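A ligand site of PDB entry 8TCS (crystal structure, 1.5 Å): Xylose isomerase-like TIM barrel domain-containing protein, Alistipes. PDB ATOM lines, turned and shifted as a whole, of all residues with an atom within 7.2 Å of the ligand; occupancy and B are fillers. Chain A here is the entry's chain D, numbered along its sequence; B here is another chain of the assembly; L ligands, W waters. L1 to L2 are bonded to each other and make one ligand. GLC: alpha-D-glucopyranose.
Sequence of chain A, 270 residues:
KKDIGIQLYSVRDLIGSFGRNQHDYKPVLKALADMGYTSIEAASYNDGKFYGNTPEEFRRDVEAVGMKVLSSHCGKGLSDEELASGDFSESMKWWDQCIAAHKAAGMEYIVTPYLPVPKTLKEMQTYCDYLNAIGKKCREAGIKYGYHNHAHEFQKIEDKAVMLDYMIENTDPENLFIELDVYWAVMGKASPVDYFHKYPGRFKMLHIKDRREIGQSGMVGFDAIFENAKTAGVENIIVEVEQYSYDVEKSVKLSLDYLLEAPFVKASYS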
ATOM      1  N   GLU A 153     -29.772  20.274 -16.608  1.00  0.00           N
ATOM      2  CA  GLU A 153     -30.289  19.250 -15.729  1.00  0.00           C
ATOM      3  C   GLU A 153     -29.165  18.294 -15.300  1.00  0.00           C
ATOM      4  O   GLU A 153     -29.381  17.434 -14.451  1.00  0.00           O
ATOM      5  CB  GLU A 153     -31.465  18.492 -16.338  1.00  0.00           C
ATOM      6  CG  GLU A 153     -32.694  19.351 -16.641  1.00  0.00           C
ATOM      7  CD  GLU A 153     -32.726  19.979 -18.010  1.00  0.00           C
ATOM      8  OE1 GLU A 153     -33.808  20.435 -18.492  1.00  0.00           O
ATOM      9  OE2 GLU A 153     -31.627  20.051 -18.599  1.00  0.00           O
ATOM     10  N   PHE A 154     -27.961  18.442 -15.888  1.00  0.00           N
ATOM     11  CA  PHE A 154     -26.822  17.632 -15.452  1.00  0.00           C
ATOM     12  C   PHE A 154     -26.081  18.340 -14.317  1.00  0.00           C
ATOM     13  O   PHE A 154     -25.127  17.769 -13.795  1.00  0.00           O
ATOM     14  CB  PHE A 154     -25.928  17.247 -16.626  1.00  0.00           C
ATOM     15  CG  PHE A 154     -26.717  16.400 -17.601  1.00  0.00           C
ATOM     16  CD1 PHE A 154     -27.041  15.078 -17.345  1.00  0.00           C
ATOM     17  CD2 PHE A 154     -27.252  16.990 -18.754  1.00  0.00           C
ATOM     18  CE1 PHE A 154     -27.849  14.353 -18.222  1.00  0.00           C
ATOM     19  CE2 PHE A 154     -28.067  16.274 -19.598  1.00  0.00           C
ATOM     20  CZ  PHE A 154     -28.370  14.973 -19.337  1.00  0.00           C
ATOM     21  N   GLN A 155     -26.525  19.544 -13.902  1.00  0.00           N
ATOM     22  CA  GLN A 155     -26.025  20.187 -12.696  1.00  0.00           C
ATOM     23  C   GLN A 155     -26.593  19.543 -11.423  1.00  0.00           C
ATOM     24  O   GLN A 155     -27.621  18.883 -11.412  1.00  0.00           O
ATOM     25  CB  GLN A 155     -26.396  21.673 -12.652  1.00  0.00           C
ATOM     26  CG  GLN A 155     -25.885  22.483 -13.841  1.00  0.00           C
ATOM     27  CD  GLN A 155     -26.404  23.909 -13.842  1.00  0.00           C
ATOM     28  OE1 GLN A 155     -26.835  24.450 -12.809  1.00  0.00           O
ATOM     29  NE2 GLN A 155     -26.402  24.532 -15.008  1.00  0.00           N
ATOM     30  N   LYS A 156     -25.841  19.697 -10.301  1.00  0.00           N
ATOM     31  CA  LYS A 156     -26.271  19.220  -9.002  1.00  0.00           C
ATOM     32  C   LYS A 156     -27.101  20.259  -8.270  1.00  0.00           C
ATOM     33  O   LYS A 156     -26.924  21.450  -8.466  1.00  0.00           O
ATOM     34  CB  LYS A 156     -25.084  18.853  -8.108  1.00  0.00           C
ATOM     35  CG  LYS A 156     -24.389  17.607  -8.642  1.00  0.00           C
ATOM     36  CD  LYS A 156     -23.123  17.170  -7.908  1.00  0.00           C
ATOM     37  CE  LYS A 156     -22.526  16.029  -8.655  1.00  0.00           C
ATOM     38  NZ  LYS A 156     -21.599  15.267  -7.820  1.00  0.00           N
ATOM     39  N   LYS A 160     -25.632  18.058  -4.236  1.00  0.00           N
ATOM     40  CA  LYS A 160     -25.978  16.689  -3.912  1.00  0.00           C
ATOM     41  C   LYS A 160     -26.431  16.033  -5.215  1.00  0.00           C
ATOM     42  O   LYS A 160     -25.611  15.820  -6.109  1.00  0.00           O
ATOM     43  CB  LYS A 160     -27.011  16.686  -2.773  1.00  0.00           C
ATOM     44  CG  LYS A 160     -26.559  17.257  -1.430  1.00  0.00           C
ATOM     45  CD  LYS A 160     -27.717  17.505  -0.457  1.00  0.00           C
ATOM     46  CE  LYS A 160     -27.337  18.045   0.904  1.00  0.00           C
ATOM     47  NZ  LYS A 160     -27.210  19.518   0.909  1.00  0.00           N
ATOM     48  N   ALA A 161     -27.737  15.826  -5.365  1.00  0.00           N
ATOM     49  CA  ALA A 161     -28.279  15.041  -6.456  1.00  0.00           C
ATOM     50  C   ALA A 161     -28.126  15.812  -7.758  1.00  0.00           C
ATOM     51  O   ALA A 161     -28.308  17.019  -7.783  1.00  0.00           O
ATOM     52  CB  ALA A 161     -29.719  14.716  -6.188  1.00  0.00           C
ATOM     53  N   VAL A 162     -27.825  15.090  -8.838  1.00  0.00           N
ATOM     54  CA  VAL A 162     -27.918  15.630 -10.178  1.00  0.00           C
ATOM     55  C   VAL A 162     -29.403  15.780 -10.472  1.00  0.00           C
ATOM     56  O   VAL A 162     -30.171  14.866 -10.187  1.00  0.00           O
ATOM     57  CB  VAL A 162     -27.247  14.709 -11.218  1.00  0.00           C
ATOM     58  CG1 VAL A 162     -27.532  15.168 -12.644  1.00  0.00           C
ATOM     59  CG2 VAL A 162     -25.751  14.636 -10.960  1.00  0.00           C
ATOM     60  N   LEU A 164     -31.412  15.747 -13.284  1.00  0.00           N
ATOM     61  CA  LEU A 164     -32.135  14.790 -14.111  1.00  0.00           C
ATOM     62  C   LEU A 164     -32.284  13.464 -13.343  1.00  0.00           C
ATOM     63  O   LEU A 164     -33.331  12.833 -13.374  1.00  0.00           O
ATOM     64  CB  LEU A 164     -31.438  14.561 -15.453  1.00  0.00           C
ATOM     65  CG  LEU A 164     -32.291  13.805 -16.477  1.00  0.00           C
ATOM     66  CD1 LEU A 164     -33.508  14.643 -16.802  1.00  0.00           C
ATOM     67  CD2 LEU A 164     -31.525  13.456 -17.742  1.00  0.00           C
ATOM     68  N   ASP A 165     -31.232  13.032 -12.630  1.00  0.00           N
ATOM     69  CA  ASP A 165     -31.275  11.769 -11.887  1.00  0.00           C
ATOM     70  C   ASP A 165     -32.381  11.813 -10.825  1.00  0.00           C
ATOM     71  O   ASP A 165     -33.200  10.885 -10.711  1.00  0.00           O
ATOM     72  CB  ASP A 165     -29.913  11.405 -11.324  1.00  0.00           C
ATOM     73  CG  ASP A 165     -28.873  11.189 -12.397  1.00  0.00           C
ATOM     74  OD1 ASP A 165     -28.605  12.180 -13.105  1.00  0.00           O
ATOM     75  OD2 ASP A 165     -28.474  10.014 -12.621  1.00  0.00           O
ATOM     76  N   GLU A 169     -35.652   9.425 -10.600  1.00  0.00           N
ATOM     77  CA  GLU A 169     -35.762   8.582  -9.398  1.00  0.00           C
ATOM     78  C   GLU A 169     -37.056   8.835  -8.644  1.00  0.00           C
ATOM     79  O   GLU A 169     -37.616   7.933  -7.977  1.00  0.00           O
ATOM     80  CB  GLU A 169     -34.553   8.836  -8.501  1.00  0.00           C
ATOM     81  CG  GLU A 169     -33.229   8.288  -9.036  1.00  0.00           C
ATOM     82  CD  GLU A 169     -31.985   8.827  -8.336  1.00  0.00           C
ATOM     83  OE1 GLU A 169     -30.860   8.473  -8.738  1.00  0.00           O
ATOM     84  OE2 GLU A 169     -32.085   9.705  -7.482  1.00  0.00           O
ATOM     85  N   ALA A 185     -27.303  16.311 -23.746  1.00  0.00           N
ATOM     86  CA  ALA A 185     -26.663  15.406 -22.786  1.00  0.00           C
ATOM     87  C   ALA A 185     -25.153  15.390 -22.949  1.00  0.00           C
ATOM     88  O   ALA A 185     -24.418  15.575 -22.010  1.00  0.00           O
ATOM     89  CB  ALA A 185     -27.216  14.014 -22.980  1.00  0.00           C
ATOM     90  N   GLY A 188     -23.625  18.456 -21.724  1.00  0.00           N
ATOM     91  CA  GLY A 188     -23.618  18.386 -20.272  1.00  0.00           C
ATOM     92  C   GLY A 188     -22.610  17.372 -19.712  1.00  0.00           C
ATOM     93  O   GLY A 188     -22.577  17.142 -18.509  1.00  0.00           O
ATOM     94  N   LYS A 189     -21.826  16.761 -20.598  1.00  0.00           N
ATOM     95  CA  LYS A 189     -20.776  15.812 -20.266  1.00  0.00           C
ATOM     96  C   LYS A 189     -21.358  14.473 -19.834  1.00  0.00           C
ATOM     97  O   LYS A 189     -20.658  13.678 -19.208  1.00  0.00           O
ATOM     98  CB  LYS A 189     -19.762  16.282 -19.230  1.00  0.00           C
ATOM     99  CG  LYS A 189     -19.094  17.583 -19.627  1.00  0.00           C
ATOM    100  CD  LYS A 189     -18.063  18.073 -18.623  1.00  0.00           C
ATOM    101  CE  LYS A 189     -17.275  19.235 -19.086  1.00  0.00           C
ATOM    102  NZ  LYS A 189     -18.100  20.445 -19.087  1.00  0.00           N
ATOM    103  N   ALA A 190     -22.613  14.200 -20.230  1.00  0.00           N
ATOM    104  CA  ALA A 190     -23.266  12.945 -19.909  1.00  0.00           C
ATOM    105  C   ALA A 190     -23.174  11.974 -21.087  1.00  0.00           C
ATOM    106  O   ALA A 190     -23.251  12.370 -22.258  1.00  0.00           O
ATOM    107  CB  ALA A 190     -24.718  13.216 -19.546  1.00  0.00           C
ATOM    108  N   SER A 191     -23.072  10.676 -20.780  1.00  0.00           N
ATOM    109  CA  SER A 191     -23.147   9.628 -21.778  1.00  0.00           C
ATOM    110  C   SER A 191     -24.595   9.185 -21.967  1.00  0.00           C
ATOM    111  O   SER A 191     -25.183   8.681 -20.998  1.00  0.00           O
ATOM    112  CB  SER A 191     -22.328   8.456 -21.349  1.00  0.00           C
ATOM    113  OG  SER A 191     -22.699   7.264 -21.992  1.00  0.00           O
ATOM    114  N   ASP A 194     -24.859   5.548 -21.001  1.00  0.00           N
ATOM    115  CA  ASP A 194     -24.778   5.261 -19.561  1.00  0.00           C
ATOM    116  C   ASP A 194     -26.088   5.607 -18.859  1.00  0.00           C
ATOM    117  O   ASP A 194     -26.511   4.853 -17.941  1.00  0.00           O
ATOM    118  CB  ASP A 194     -23.564   5.917 -18.904  1.00  0.00           C
ATOM    119  CG  ASP A 194     -22.219   5.303 -19.283  1.00  0.00           C
ATOM    120  OD1 ASP A 194     -22.213   4.158 -19.805  1.00  0.00           O
ATOM    121  OD2 ASP A 194     -21.166   5.985 -19.044  1.00  0.00           O
ATOM    122  N   TYR A 195     -26.748   6.695 -19.287  1.00  0.00           N
ATOM    123  CA  TYR A 195     -28.086   7.029 -18.765  1.00  0.00           C
ATOM    124  C   TYR A 195     -29.092   5.905 -19.083  1.00  0.00           C
ATOM    125  O   TYR A 195     -29.892   5.512 -18.206  1.00  0.00           O
ATOM    126  CB  TYR A 195     -28.585   8.399 -19.193  1.00  0.00           C
ATOM    127  CG  TYR A 195     -28.224   9.453 -18.162  1.00  0.00           C
ATOM    128  CD1 TYR A 195     -26.951  10.024 -18.128  1.00  0.00           C
ATOM    129  CD2 TYR A 195     -29.107   9.863 -17.181  1.00  0.00           C
ATOM    130  CE1 TYR A 195     -26.577  10.912 -17.142  1.00  0.00           C
ATOM    131  CE2 TYR A 195     -28.771  10.764 -16.188  1.00  0.00           C
ATOM    132  CZ  TYR A 195     -27.480  11.297 -16.152  1.00  0.00           C
ATOM    133  OH  TYR A 195     -27.140  12.207 -15.179  1.00  0.00           O
ATOM    134  N   LYS A 198     -28.527   3.084 -16.651  1.00  0.00           N
ATOM    135  CA  LYS A 198     -28.845   3.453 -15.286  1.00  0.00           C
ATOM    136  C   LYS A 198     -30.365   3.492 -15.034  1.00  0.00           C
ATOM    137  O   LYS A 198     -30.803   3.159 -13.926  1.00  0.00           O
ATOM    138  CB  LYS A 198     -28.275   4.836 -14.939  1.00  0.00           C
ATOM    139  CG  LYS A 198     -28.168   5.193 -13.488  1.00  0.00           C
ATOM    140  CD  LYS A 198     -27.033   6.208 -13.346  1.00  0.00           C
ATOM    141  CE  LYS A 198     -27.116   7.059 -12.146  1.00  0.00           C
ATOM    142  NZ  LYS A 198     -27.451   6.290 -10.950  1.00  0.00           N
ATOM    143  N   TYR A 199     -31.128   3.869 -16.080  1.00  0.00           N
ATOM    144  CA  TYR A 199     -32.573   4.078 -15.937  1.00  0.00           C
ATOM    145  C   TYR A 199     -33.276   3.357 -17.079  1.00  0.00           C
ATOM    146  O   TYR A 199     -33.976   3.945 -17.925  1.00  0.00           O
ATOM    147  CB  TYR A 199     -32.989   5.565 -15.823  1.00  0.00           C
ATOM    148  CG  TYR A 199     -32.265   6.337 -14.763  1.00  0.00           C
ATOM    149  CD1 TYR A 199     -32.540   6.101 -13.422  1.00  0.00           C
ATOM    150  CD2 TYR A 199     -31.231   7.222 -15.046  1.00  0.00           C
ATOM    151  CE1 TYR A 199     -31.856   6.754 -12.418  1.00  0.00           C
ATOM    152  CE2 TYR A 199     -30.551   7.901 -14.056  1.00  0.00           C
ATOM    153  CZ  TYR A 199     -30.847   7.649 -12.734  1.00  0.00           C
ATOM    154  OH  TYR A 199     -30.162   8.267 -11.726  1.00  0.00           O
ATOM    155  N   ARG B 211     -15.315   7.637 -23.693  1.00  0.00           N
ATOM    156  CA  ARG B 211     -15.283   7.660 -22.235  1.00  0.00           C
ATOM    157  C   ARG B 211     -14.599   6.392 -21.693  1.00  0.00           C
ATOM    158  O   ARG B 211     -13.752   6.451 -20.801  1.00  0.00           O
ATOM    159  CB  ARG B 211     -16.740   7.789 -21.738  1.00  0.00           C
ATOM    160  CG  ARG B 211     -16.887   7.781 -20.218  1.00  0.00           C
ATOM    161  CD  ARG B 211     -18.026   8.641 -19.667  1.00  0.00           C
ATOM    162  NE  ARG B 211     -17.765  10.049 -19.959  1.00  0.00           N
ATOM    163  CZ  ARG B 211     -18.564  11.040 -19.622  1.00  0.00           C
ATOM    164  NH1 ARG B 211     -19.718  10.772 -19.022  1.00  0.00           N
ATOM    165  NH2 ARG B 211     -18.232  12.295 -19.876  1.00  0.00           N
ATOM    166  N   MET B 219     -21.129   9.486 -27.025  1.00  0.00           N
ATOM    167  CA  MET B 219     -20.643  10.858 -26.943  1.00  0.00           C
ATOM    168  C   MET B 219     -19.751  11.270 -28.117  1.00  0.00           C
ATOM    169  O   MET B 219     -19.394  12.456 -28.164  1.00  0.00           O
ATOM    170  CB  MET B 219     -19.846  11.084 -25.655  1.00  0.00           C
ATOM    171  CG  MET B 219     -20.607  10.762 -24.410  1.00  0.00           C
ATOM    172  SD  MET B 219     -19.736  11.205 -22.891  1.00  0.00           S
ATOM    173  CE  MET B 219     -19.822  12.995 -23.033  1.00  0.00           C
ATOM    174  N   GLN B 243     -10.220   4.475 -19.141  1.00  0.00           N
ATOM    175  CA  GLN B 243     -11.236   4.001 -18.214  1.00  0.00           C
ATOM    176  C   GLN B 243     -11.925   2.813 -18.863  1.00  0.00           C
ATOM    177  O   GLN B 243     -12.006   2.757 -20.090  1.00  0.00           O
ATOM    178  CB  GLN B 243     -12.259   5.050 -17.799  1.00  0.00           C
ATOM    179  CG  GLN B 243     -11.711   6.340 -17.213  1.00  0.00           C
ATOM    180  CD  GLN B 243     -12.831   7.334 -16.919  1.00  0.00           C
ATOM    181  OE1 GLN B 243     -13.419   7.976 -17.823  1.00  0.00           O
ATOM    182  NE2 GLN B 243     -13.190   7.397 -15.651  1.00  0.00           N
HETATM  183  C1  GLC L   1     -21.333  11.074 -10.960  1.00  0.00           C
HETATM  184  C2  GLC L   1     -21.147  12.279 -10.048  1.00  0.00           C
HETATM  185  C3  GLC L   1     -19.781  12.946 -10.296  1.00  0.00           C
HETATM  186  C4  GLC L   1     -18.631  11.946 -10.216  1.00  0.00           C
HETATM  187  C5  GLC L   1     -18.930  10.705 -11.086  1.00  0.00           C
HETATM  188  C6  GLC L   1     -17.932   9.588 -10.861  1.00  0.00           C
HETATM  189  O2  GLC L   1     -22.200  13.240 -10.214  1.00  0.00           O
HETATM  190  O3  GLC L   1     -19.593  13.994  -9.336  1.00  0.00           O
HETATM  191  O4  GLC L   1     -17.401  12.551 -10.658  1.00  0.00           O
HETATM  192  O5  GLC L   1     -20.236  10.163 -10.775  1.00  0.00           O
HETATM  193  O6  GLC L   1     -17.652   8.898 -12.062  1.00  0.00           O
HETATM  194  C1  GLC L   2     -21.761  10.466 -13.191  1.00  0.00           C
HETATM  195  C2  GLC L   2     -21.616  10.890 -14.658  1.00  0.00           C
HETATM  196  C3  GLC L   2     -22.562  12.079 -14.983  1.00  0.00           C
HETATM  197  C4  GLC L   2     -24.011  11.793 -14.532  1.00  0.00           C
HETATM  198  C5  GLC L   2     -24.086  11.292 -13.079  1.00  0.00           C
HETATM  199  C6  GLC L   2     -25.469  10.755 -12.724  1.00  0.00           C
HETATM  200  O1  GLC L   2     -21.367  11.459 -12.307  1.00  0.00           O
HETATM  201  O2  GLC L   2     -20.273  11.227 -15.071  1.00  0.00           O
HETATM  202  O3  GLC L   2     -22.511  12.316 -16.389  1.00  0.00           O
HETATM  203  O4  GLC L   2     -24.746  12.985 -14.656  1.00  0.00           O
HETATM  204  O5  GLC L   2     -23.139  10.187 -12.891  1.00  0.00           O
HETATM  205  O6  GLC L   2     -25.889   9.630 -13.565  1.00  0.00           O
HETATM  206  O   HOH W   1     -19.388  13.652 -16.852  1.00  0.00           O
HETATM  207  O   HOH W   2     -24.818   8.274 -16.205  1.00  0.00           O
HETATM  208  O   HOH W   3     -23.167   9.966 -17.885  1.00  0.00           O
HETATM  209  O   HOH W   4     -19.185   7.986 -15.710  1.00  0.00           O
HETATM  210  O   HOH W   5     -22.419  14.992 -16.659  1.00  0.00           O
HETATM  211  O   HOH W   6     -23.741  15.374 -14.226  1.00  0.00           O
HETATM  212  O   HOH W   7     -15.329   7.875 -14.243  1.00  0.00           O
HETATM  213  O   HOH W   8     -22.019  15.092 -12.231  1.00  0.00           O
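Water W6 bridges O4 of GLC L2 (2.6 Å) and O of Phe 154 (2.8 Å).
Water W5 lies within hydrogen-bond range of an oxygen (O3) of GLC L2 (2.7 Å), the backbone carbonyl oxygen of Gly 188 (2.8 Å) and the backbone carbonyl oxygen of Lys 189 (3.4 Å).
Water W3 bridges an oxygen (O3) of GLC L2 and the backbone NH of Ser 191.
Water W1 lies within hydrogen-bond range of O of Lys 189 (2.7 Å) and O2 of GLC L2 (3.1 Å).
OH of Tyr 195 sits at hydrogen-bond distance from O4 of GLC L2, at 2.6 Å.
OD2 of Asp 165 sits at hydrogen-bond distance from O6 of GLC L2, at 2.8 Å.
The side-chain amino group (NZ) of Lys 156 lies within hydrogen-bond range of an oxygen (O3) of GLC L1, 2.8 Å away.
Val 162 touches the ligand.
O of Lys 189 touches O3 of GLC L2 (3.6 Å).
CA of Ala 190 touches O3 of GLC L2, at 3.7 Å.
CE of Lys 198 touches O6 of GLC L2, 3.2 Å away.
Hydrophobic or aromatic side chains that line the ligand: Val 162, Ala 190 and Tyr 195.
OD1 of Asp 165 sits at hydrogen-bond distance from OH of Tyr 195, at 2.5 Å.
The side-chain carboxylate of Asp 165 lies within hydrogen-bond range of the side-chain hydroxyl of Tyr 199.
The side-chain amino group (NZ) of Lys 198 sits close to the side-chain hydroxyl (OH) of Tyr 199 (3.4 Å).
The backbone carbonyl oxygen (O) of Lys 189 sits at hydrogen-bond distance from the guanidinium group (NH2) of Arg 211 of chain B, at 2.9 Å.
O of Ala 185 is in hydrogen-bond range of N of Ala 190, at 2.9 Å.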
